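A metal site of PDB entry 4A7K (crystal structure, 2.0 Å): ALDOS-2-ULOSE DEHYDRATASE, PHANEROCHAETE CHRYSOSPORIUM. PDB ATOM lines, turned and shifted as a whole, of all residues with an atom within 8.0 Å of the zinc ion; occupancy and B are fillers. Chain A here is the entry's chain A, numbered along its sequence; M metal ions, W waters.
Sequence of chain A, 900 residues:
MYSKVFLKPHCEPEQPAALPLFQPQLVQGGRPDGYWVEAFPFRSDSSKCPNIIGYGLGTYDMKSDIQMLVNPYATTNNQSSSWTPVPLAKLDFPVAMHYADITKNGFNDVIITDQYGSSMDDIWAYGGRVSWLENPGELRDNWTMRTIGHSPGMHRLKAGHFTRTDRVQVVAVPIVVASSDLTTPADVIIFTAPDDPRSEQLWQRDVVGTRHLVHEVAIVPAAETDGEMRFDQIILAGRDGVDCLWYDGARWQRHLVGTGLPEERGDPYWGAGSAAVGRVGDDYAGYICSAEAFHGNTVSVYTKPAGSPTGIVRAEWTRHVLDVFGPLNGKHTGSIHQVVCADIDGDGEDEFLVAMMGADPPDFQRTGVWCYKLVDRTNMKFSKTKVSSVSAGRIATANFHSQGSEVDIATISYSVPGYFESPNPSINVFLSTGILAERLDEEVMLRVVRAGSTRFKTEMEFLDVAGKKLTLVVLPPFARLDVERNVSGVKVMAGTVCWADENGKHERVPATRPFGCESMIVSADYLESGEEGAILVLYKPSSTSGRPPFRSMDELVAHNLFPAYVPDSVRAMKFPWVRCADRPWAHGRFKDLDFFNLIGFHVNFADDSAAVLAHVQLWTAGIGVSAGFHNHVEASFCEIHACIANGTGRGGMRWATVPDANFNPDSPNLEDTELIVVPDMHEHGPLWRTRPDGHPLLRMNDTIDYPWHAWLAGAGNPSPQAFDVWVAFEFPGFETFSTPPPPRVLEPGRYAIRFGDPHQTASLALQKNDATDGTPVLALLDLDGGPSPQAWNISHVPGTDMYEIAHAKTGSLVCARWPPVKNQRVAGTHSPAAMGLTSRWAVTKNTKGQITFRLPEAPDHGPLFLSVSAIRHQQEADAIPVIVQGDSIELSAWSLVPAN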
ATOM      1  N   TYR A  35       4.049   6.825 -18.212  1.00  0.00           N
ATOM      2  CA  TYR A  35       3.403   6.822 -19.501  1.00  0.00           C
ATOM      3  C   TYR A  35       4.042   7.741 -20.502  1.00  0.00           C
ATOM      4  O   TYR A  35       4.300   7.365 -21.609  1.00  0.00           O
ATOM      5  CB  TYR A  35       1.900   7.201 -19.368  1.00  0.00           C
ATOM      6  CG  TYR A  35       1.120   7.076 -20.702  1.00  0.00           C
ATOM      7  CD1 TYR A  35       0.660   5.835 -21.118  1.00  0.00           C
ATOM      8  CD2 TYR A  35       0.829   8.205 -21.503  1.00  0.00           C
ATOM      9  CE1 TYR A  35      -0.069   5.675 -22.304  1.00  0.00           C
ATOM     10  CE2 TYR A  35       0.101   8.068 -22.704  1.00  0.00           C
ATOM     11  CZ  TYR A  35      -0.319   6.786 -23.105  1.00  0.00           C
ATOM     12  OH  TYR A  35      -1.093   6.576 -24.278  1.00  0.00           O
ATOM     13  N   TRP A  36       4.340   8.977 -20.102  1.00  0.00           N
ATOM     14  CA  TRP A  36       4.779   9.966 -21.080  1.00  0.00           C
ATOM     15  C   TRP A  36       6.088  10.573 -20.692  1.00  0.00           C
ATOM     16  O   TRP A  36       6.310  10.882 -19.494  1.00  0.00           O
ATOM     17  CB  TRP A  36       3.740  11.103 -21.144  1.00  0.00           C
ATOM     18  CG  TRP A  36       3.809  11.925 -22.415  1.00  0.00           C
ATOM     19  CD1 TRP A  36       4.575  13.047 -22.655  1.00  0.00           C
ATOM     20  CD2 TRP A  36       3.075  11.672 -23.687  1.00  0.00           C
ATOM     21  NE1 TRP A  36       4.417  13.486 -23.954  1.00  0.00           N
ATOM     22  CE2 TRP A  36       3.498  12.747 -24.618  1.00  0.00           C
ATOM     23  CE3 TRP A  36       2.167  10.691 -24.121  1.00  0.00           C
ATOM     24  CZ2 TRP A  36       3.017  12.831 -25.920  1.00  0.00           C
ATOM     25  CZ3 TRP A  36       1.683  10.769 -25.447  1.00  0.00           C
ATOM     26  CH2 TRP A  36       2.082  11.823 -26.319  1.00  0.00           C
ATOM     27  N   LEU A  57      -0.504   7.902 -16.171  1.00  0.00           N
ATOM     28  CA  LEU A  57      -1.942   8.085 -16.354  1.00  0.00           C
ATOM     29  C   LEU A  57      -2.691   8.444 -15.071  1.00  0.00           C
ATOM     30  O   LEU A  57      -3.851   8.823 -15.163  1.00  0.00           O
ATOM     31  CB  LEU A  57      -2.590   6.867 -17.015  1.00  0.00           C
ATOM     32  CG  LEU A  57      -1.957   6.631 -18.402  1.00  0.00           C
ATOM     33  CD1 LEU A  57      -2.412   5.306 -19.052  1.00  0.00           C
ATOM     34  CD2 LEU A  57      -2.201   7.808 -19.352  1.00  0.00           C
ATOM     35  N   VAL A  95      -3.121  12.358 -20.511  1.00  0.00           N
ATOM     36  CA  VAL A  95      -2.620  11.493 -21.551  1.00  0.00           C
ATOM     37  C   VAL A  95      -1.446  12.101 -22.326  1.00  0.00           C
ATOM     38  O   VAL A  95      -0.271  11.796 -22.002  1.00  0.00           O
ATOM     39  CB  VAL A  95      -3.722  10.789 -22.413  1.00  0.00           C
ATOM     40  CG1 VAL A  95      -3.071   9.744 -23.358  1.00  0.00           C
ATOM     41  CG2 VAL A  95      -4.746  10.149 -21.504  1.00  0.00           C
ATOM     42  N   TYR A 116      -9.282  11.983 -19.226  1.00  0.00           N
ATOM     43  CA  TYR A 116      -9.489  10.878 -20.181  1.00  0.00           C
ATOM     44  C   TYR A 116     -10.410   9.836 -19.561  1.00  0.00           C
ATOM     45  O   TYR A 116     -11.421   9.416 -20.182  1.00  0.00           O
ATOM     46  CB  TYR A 116      -8.111  10.257 -20.583  1.00  0.00           C
ATOM     47  CG  TYR A 116      -8.152   9.030 -21.497  1.00  0.00           C
ATOM     48  CD1 TYR A 116      -8.441   9.152 -22.863  1.00  0.00           C
ATOM     49  CD2 TYR A 116      -7.871   7.757 -20.988  1.00  0.00           C
ATOM     50  CE1 TYR A 116      -8.480   8.022 -23.700  1.00  0.00           C
ATOM     51  CE2 TYR A 116      -7.896   6.627 -21.798  1.00  0.00           C
ATOM     52  CZ  TYR A 116      -8.206   6.758 -23.163  1.00  0.00           C
ATOM     53  OH  TYR A 116      -8.248   5.642 -24.017  1.00  0.00           O
ATOM     54  N   MET A 120      -9.774   2.557 -21.943  1.00  0.00           N
ATOM     55  CA  MET A 120     -10.736   2.466 -23.014  1.00  0.00           C
ATOM     56  C   MET A 120     -12.099   1.933 -22.589  1.00  0.00           C
ATOM     57  O   MET A 120     -13.068   2.152 -23.328  1.00  0.00           O
ATOM     58  CB  MET A 120     -10.181   1.681 -24.206  1.00  0.00           C
ATOM     59  CG  MET A 120      -9.034   2.408 -24.908  1.00  0.00           C
ATOM     60  SD  MET A 120      -8.354   1.452 -26.319  1.00  0.00           S
ATOM     61  CE  MET A 120      -9.200   2.228 -27.673  1.00  0.00           C
ATOM     62  N   HIS A 155      -6.719  11.753 -26.877  1.00  0.00           N
ATOM     63  CA  HIS A 155      -5.623  10.808 -26.601  1.00  0.00           C
ATOM     64  C   HIS A 155      -4.230  11.150 -27.136  1.00  0.00           C
ATOM     65  O   HIS A 155      -3.232  10.686 -26.592  1.00  0.00           O
ATOM     66  CB  HIS A 155      -6.148   9.386 -26.952  1.00  0.00           C
ATOM     67  CG  HIS A 155      -5.095   8.300 -26.965  1.00  0.00           C
ATOM     68  ND1 HIS A 155      -4.278   8.104 -28.017  1.00  0.00           N
ATOM     69  CD2 HIS A 155      -4.811   7.274 -26.037  1.00  0.00           C
ATOM     70  CE1 HIS A 155      -3.461   7.043 -27.772  1.00  0.00           C
ATOM     71  NE2 HIS A 155      -3.783   6.537 -26.566  1.00  0.00           N
ATOM     72  N   ARG A 156      -4.148  11.914 -28.228  1.00  0.00           N
ATOM     73  CA  ARG A 156      -2.882  12.345 -28.773  1.00  0.00           C
ATOM     74  C   ARG A 156      -3.069  13.757 -29.238  1.00  0.00           C
ATOM     75  O   ARG A 156      -4.187  14.162 -29.586  1.00  0.00           O
ATOM     76  CB  ARG A 156      -2.409  11.471 -29.952  1.00  0.00           C
ATOM     77  CG  ARG A 156      -1.916  10.100 -29.537  1.00  0.00           C
ATOM     78  CD  ARG A 156      -0.609  10.250 -28.773  1.00  0.00           C
ATOM     79  NE  ARG A 156      -0.067   8.934 -28.415  1.00  0.00           N
ATOM     80  CZ  ARG A 156      -0.402   8.272 -27.290  1.00  0.00           C
ATOM     81  NH1 ARG A 156      -1.280   8.787 -26.411  1.00  0.00           N
ATOM     82  NH2 ARG A 156       0.148   7.087 -27.072  1.00  0.00           N
ATOM     83  N   ILE A 175      -8.964   8.610 -29.246  1.00  0.00           N
ATOM     84  CA  ILE A 175      -8.789   7.228 -29.723  1.00  0.00           C
ATOM     85  C   ILE A 175     -10.105   6.460 -29.858  1.00  0.00           C
ATOM     86  O   ILE A 175     -10.276   5.666 -30.789  1.00  0.00           O
ATOM     87  CB  ILE A 175      -7.734   6.464 -28.841  1.00  0.00           C
ATOM     88  CG1 ILE A 175      -7.389   5.066 -29.391  1.00  0.00           C
ATOM     89  CG2 ILE A 175      -8.145   6.334 -27.349  1.00  0.00           C
ATOM     90  CD1 ILE A 175      -6.043   4.519 -28.843  1.00  0.00           C
ATOM     91  N   VAL A 214      -7.002   6.048 -33.672  1.00  0.00           N
ATOM     92  CA  VAL A 214      -5.736   6.750 -33.799  1.00  0.00           C
ATOM     93  C   VAL A 214      -4.911   6.718 -32.502  1.00  0.00           C
ATOM     94  O   VAL A 214      -5.362   7.143 -31.393  1.00  0.00           O
ATOM     95  CB  VAL A 214      -5.965   8.165 -34.235  1.00  0.00           C
ATOM     96  CG1 VAL A 214      -4.660   8.963 -34.120  1.00  0.00           C
ATOM     97  CG2 VAL A 214      -6.523   8.136 -35.658  1.00  0.00           C
ATOM     98  N   HIS A 215      -3.677   6.243 -32.618  1.00  0.00           N
ATOM     99  CA  HIS A 215      -2.862   6.027 -31.446  1.00  0.00           C
ATOM    100  C   HIS A 215      -1.629   6.867 -31.525  1.00  0.00           C
ATOM    101  O   HIS A 215      -0.875   6.923 -30.564  1.00  0.00           O
ATOM    102  CB  HIS A 215      -2.507   4.545 -31.318  1.00  0.00           C
ATOM    103  CG  HIS A 215      -1.764   4.175 -30.024  1.00  0.00           C
ATOM    104  ND1 HIS A 215      -0.432   3.981 -29.971  1.00  0.00           N
ATOM    105  CD2 HIS A 215      -2.233   4.020 -28.697  1.00  0.00           C
ATOM    106  CE1 HIS A 215      -0.077   3.715 -28.703  1.00  0.00           C
ATOM    107  NE2 HIS A 215      -1.187   3.732 -27.945  1.00  0.00           N
ATOM    108  N   GLU A 216      -1.335   7.444 -32.696  1.00  0.00           N
ATOM    109  CA  GLU A 216      -0.154   8.335 -32.749  1.00  0.00           C
ATOM    110  C   GLU A 216      -0.450   9.448 -33.711  1.00  0.00           C
ATOM    111  O   GLU A 216      -1.056   9.168 -34.760  1.00  0.00           O
ATOM    112  CB  GLU A 216       1.118   7.601 -33.260  1.00  0.00           C
ATOM    113  CG  GLU A 216       2.415   8.296 -32.838  1.00  0.00           C
ATOM    114  CD  GLU A 216       2.677   8.035 -31.363  1.00  0.00           C
ATOM    115  OE1 GLU A 216       3.268   6.980 -31.105  1.00  0.00           O
ATOM    116  OE2 GLU A 216       2.237   8.811 -30.467  1.00  0.00           O
ATOM    117  N   GLY A 273      -0.211   1.208 -34.797  1.00  0.00           N
ATOM    118  CA  GLY A 273      -0.185   1.707 -33.445  1.00  0.00           C
ATOM    119  C   GLY A 273       0.629   3.037 -33.408  1.00  0.00           C
ATOM    120  O   GLY A 273       0.332   3.883 -32.579  1.00  0.00           O
ATOM    121  N   PHE A 294      -2.401  -1.414 -32.609  1.00  0.00           N
ATOM    122  CA  PHE A 294      -2.458  -0.735 -31.266  1.00  0.00           C
ATOM    123  C   PHE A 294      -1.679  -1.617 -30.293  1.00  0.00           C
ATOM    124  O   PHE A 294      -2.012  -2.842 -30.146  1.00  0.00           O
ATOM    125  CB  PHE A 294      -3.953  -0.543 -30.828  1.00  0.00           C
ATOM    126  CG  PHE A 294      -4.150  -0.254 -29.358  1.00  0.00           C
ATOM    127  CD1 PHE A 294      -4.087   1.036 -28.881  1.00  0.00           C
ATOM    128  CD2 PHE A 294      -4.407  -1.307 -28.462  1.00  0.00           C
ATOM    129  CE1 PHE A 294      -4.258   1.296 -27.499  1.00  0.00           C
ATOM    130  CE2 PHE A 294      -4.584  -1.063 -27.106  1.00  0.00           C
ATOM    131  CZ  PHE A 294      -4.506   0.252 -26.615  1.00  0.00           C
ATOM    132  N   HIS A 295      -0.638  -1.072 -29.697  1.00  0.00           N
ATOM    133  CA  HIS A 295       0.155  -1.843 -28.703  1.00  0.00           C
ATOM    134  C   HIS A 295       0.687  -3.142 -29.203  1.00  0.00           C
ATOM    135  O   HIS A 295       0.843  -4.088 -28.423  1.00  0.00           O
ATOM    136  CB  HIS A 295      -0.666  -2.115 -27.413  1.00  0.00           C
ATOM    137  CG  HIS A 295      -0.933  -0.870 -26.608  1.00  0.00           C
ATOM    138  ND1 HIS A 295      -1.249  -0.905 -25.268  1.00  0.00           N
ATOM    139  CD2 HIS A 295      -0.962   0.493 -26.983  1.00  0.00           C
ATOM    140  CE1 HIS A 295      -1.400   0.386 -24.842  1.00  0.00           C
ATOM    141  NE2 HIS A 295      -1.285   1.206 -25.884  1.00  0.00           N
ATOM    142  N   ILE A 336       4.861  -3.044 -28.099  1.00  0.00           N
ATOM    143  CA  ILE A 336       5.458  -1.873 -28.728  1.00  0.00           C
ATOM    144  C   ILE A 336       4.517  -0.749 -28.566  1.00  0.00           C
ATOM    145  O   ILE A 336       3.376  -0.888 -28.963  1.00  0.00           O
ATOM    146  CB  ILE A 336       5.700  -2.046 -30.211  1.00  0.00           C
ATOM    147  CG1 ILE A 336       6.547  -3.309 -30.485  1.00  0.00           C
ATOM    148  CG2 ILE A 336       6.305  -0.743 -30.798  1.00  0.00           C
ATOM    149  CD1 ILE A 336       6.611  -3.660 -31.968  1.00  0.00           C
ATOM    150  N   HIS A 337       4.977   0.380 -28.007  1.00  0.00           N
ATOM    151  CA  HIS A 337       4.110   1.495 -27.786  1.00  0.00           C
ATOM    152  C   HIS A 337       4.260   2.649 -28.752  1.00  0.00           C
ATOM    153  O   HIS A 337       3.295   3.366 -28.987  1.00  0.00           O
ATOM    154  CB  HIS A 337       4.282   2.065 -26.379  1.00  0.00           C
ATOM    155  CG  HIS A 337       3.050   2.833 -25.906  1.00  0.00           C
ATOM    156  ND1 HIS A 337       3.111   4.120 -25.407  1.00  0.00           N
ATOM    157  CD2 HIS A 337       1.701   2.501 -26.004  1.00  0.00           C
ATOM    158  CE1 HIS A 337       1.855   4.535 -25.134  1.00  0.00           C
ATOM    159  NE2 HIS A 337       1.002   3.503 -25.471  1.00  0.00           N
ATOM    160  N   GLN A 338       5.458   2.829 -29.332  1.00  0.00           N
ATOM    161  CA  GLN A 338       5.801   4.027 -30.134  1.00  0.00           C
ATOM    162  C   GLN A 338       7.006   3.764 -31.046  1.00  0.00           C
ATOM    163  O   GLN A 338       7.900   2.998 -30.664  1.00  0.00           O
ATOM    164  CB  GLN A 338       6.236   5.099 -29.168  1.00  0.00           C
ATOM    165  CG  GLN A 338       6.364   6.518 -29.687  1.00  0.00           C
ATOM    166  CD  GLN A 338       7.250   7.355 -28.740  1.00  0.00           C
ATOM    167  OE1 GLN A 338       7.926   6.786 -27.858  1.00  0.00           O
ATOM    168  NE2 GLN A 338       7.269   8.710 -28.923  1.00  0.00           N
ATOM    169  N   MET A 357       7.567  -1.761 -24.149  1.00  0.00           N
ATOM    170  CA  MET A 357       7.035  -1.617 -22.800  1.00  0.00           C
ATOM    171  C   MET A 357       7.434  -2.693 -21.799  1.00  0.00           C
ATOM    172  O   MET A 357       7.406  -2.423 -20.582  1.00  0.00           O
ATOM    173  CB  MET A 357       5.486  -1.634 -22.883  1.00  0.00           C
ATOM    174  CG  MET A 357       4.939  -0.574 -23.865  1.00  0.00           C
ATOM    175  SD  MET A 357       3.124  -0.723 -24.057  1.00  0.00           S
ATOM    176  CE  MET A 357       3.001  -1.703 -25.509  1.00  0.00           C
ATOM    177  N   GLY A 393       7.770   2.998 -22.202  1.00  0.00           N
ATOM    178  CA  GLY A 393       6.425   3.354 -22.735  1.00  0.00           C
ATOM    179  C   GLY A 393       6.452   4.574 -23.709  1.00  0.00           C
ATOM    180  O   GLY A 393       5.515   4.809 -24.488  1.00  0.00           O
ATOM    181  N   ARG A 394       7.502   5.387 -23.623  1.00  0.00           N
ATOM    182  CA  ARG A 394       7.670   6.506 -24.552  1.00  0.00           C
ATOM    183  C   ARG A 394       9.108   6.907 -24.578  1.00  0.00           C
ATOM    184  O   ARG A 394       9.833   6.703 -23.569  1.00  0.00           O
ATOM    185  CB  ARG A 394       6.816   7.732 -24.175  1.00  0.00           C
ATOM    186  CG  ARG A 394       6.529   8.611 -25.400  1.00  0.00           C
ATOM    187  CD  ARG A 394       5.372   9.662 -25.176  1.00  0.00           C
ATOM    188  NE  ARG A 394       4.932  10.114 -26.484  1.00  0.00           N
ATOM    189  CZ  ARG A 394       4.193   9.371 -27.321  1.00  0.00           C
ATOM    190  NH1 ARG A 394       3.770   8.121 -26.989  1.00  0.00           N
ATOM    191  NH2 ARG A 394       3.906   9.888 -28.487  1.00  0.00           N
ATOM    192  N   TYR A 414       6.715   2.000 -18.946  1.00  0.00           N
ATOM    193  CA  TYR A 414       5.316   1.958 -19.131  1.00  0.00           C
ATOM    194  C   TYR A 414       4.796   1.252 -17.857  1.00  0.00           C
ATOM    195  O   TYR A 414       5.095   0.085 -17.636  1.00  0.00           O
ATOM    196  CB  TYR A 414       5.000   1.136 -20.375  1.00  0.00           C
ATOM    197  CG  TYR A 414       3.526   1.120 -20.656  1.00  0.00           C
ATOM    198  CD1 TYR A 414       2.720   0.140 -20.106  1.00  0.00           C
ATOM    199  CD2 TYR A 414       2.952   2.064 -21.475  1.00  0.00           C
ATOM    200  CE1 TYR A 414       1.345   0.128 -20.334  1.00  0.00           C
ATOM    201  CE2 TYR A 414       1.585   2.071 -21.701  1.00  0.00           C
ATOM    202  CZ  TYR A 414       0.781   1.097 -21.126  1.00  0.00           C
ATOM    203  OH  TYR A 414      -0.599   1.064 -21.349  1.00  0.00           O
ATOM    204  N   TYR A 419      -3.087  -2.751 -14.379  1.00  0.00           N
ATOM    205  CA  TYR A 419      -3.187  -3.131 -15.796  1.00  0.00           C
ATOM    206  C   TYR A 419      -1.893  -3.792 -16.335  1.00  0.00           C
ATOM    207  O   TYR A 419      -1.846  -5.009 -16.414  1.00  0.00           O
ATOM    208  CB  TYR A 419      -3.755  -1.981 -16.672  1.00  0.00           C
ATOM    209  CG  TYR A 419      -3.658  -2.232 -18.179  1.00  0.00           C
ATOM    210  CD1 TYR A 419      -4.641  -2.996 -18.860  1.00  0.00           C
ATOM    211  CD2 TYR A 419      -2.608  -1.665 -18.920  1.00  0.00           C
ATOM    212  CE1 TYR A 419      -4.537  -3.195 -20.229  1.00  0.00           C
ATOM    213  CE2 TYR A 419      -2.473  -1.858 -20.276  1.00  0.00           C
ATOM    214  CZ  TYR A 419      -3.433  -2.625 -20.933  1.00  0.00           C
ATOM    215  OH  TYR A 419      -3.265  -2.787 -22.293  1.00  0.00           O
HETATM  216 ZN    ZN M   1      -1.054   3.319 -25.884  1.00  0.00          ZN
HETATM  217  O   HOH W   1      -2.442   4.461 -24.954  1.00  0.00           O
HETATM  218  O   HOH W   2      -1.715   3.025 -23.043  1.00  0.00           O
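Water W1 bridges the side-chain hydroxyl of Tyr 35 (2.6 Å) and a ring nitrogen (NE2) of His 155 (3.0 Å).
A ring nitrogen (ND1) of His 337 is in hydrogen-bond range of the backbone carbonyl oxygen of Gly 393, 2.7 Å away.
NH1 of Arg 156 sits at hydrogen-bond distance from OH of Tyr 35 (3.1 Å).
The guanidinium group (NE) of Arg 156 lies within hydrogen-bond range of the backbone carbonyl oxygen (O) of His 215, at 3.1 Å.
A ring nitrogen (ND1) of His 215 is in hydrogen-bond range of the backbone carbonyl oxygen of Gly 273 (2.7 Å).
Merely in contact with the zinc ion: Tyr 35.
Of the 23 residues printed, 4 come within 4 Å of the zinc ion.
The nearest printed residue that does not touch the zinc ion is Phe 294 (4.1 Å).
The zinc ion is bound by water W1 (2.0 Å), NE2 of His 337 (2.1 Å), NE2 of His 215 (2.1 Å) and NE2 of His 295 (2.1 Å).
The zinc ion has four donor atoms within binding distance.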
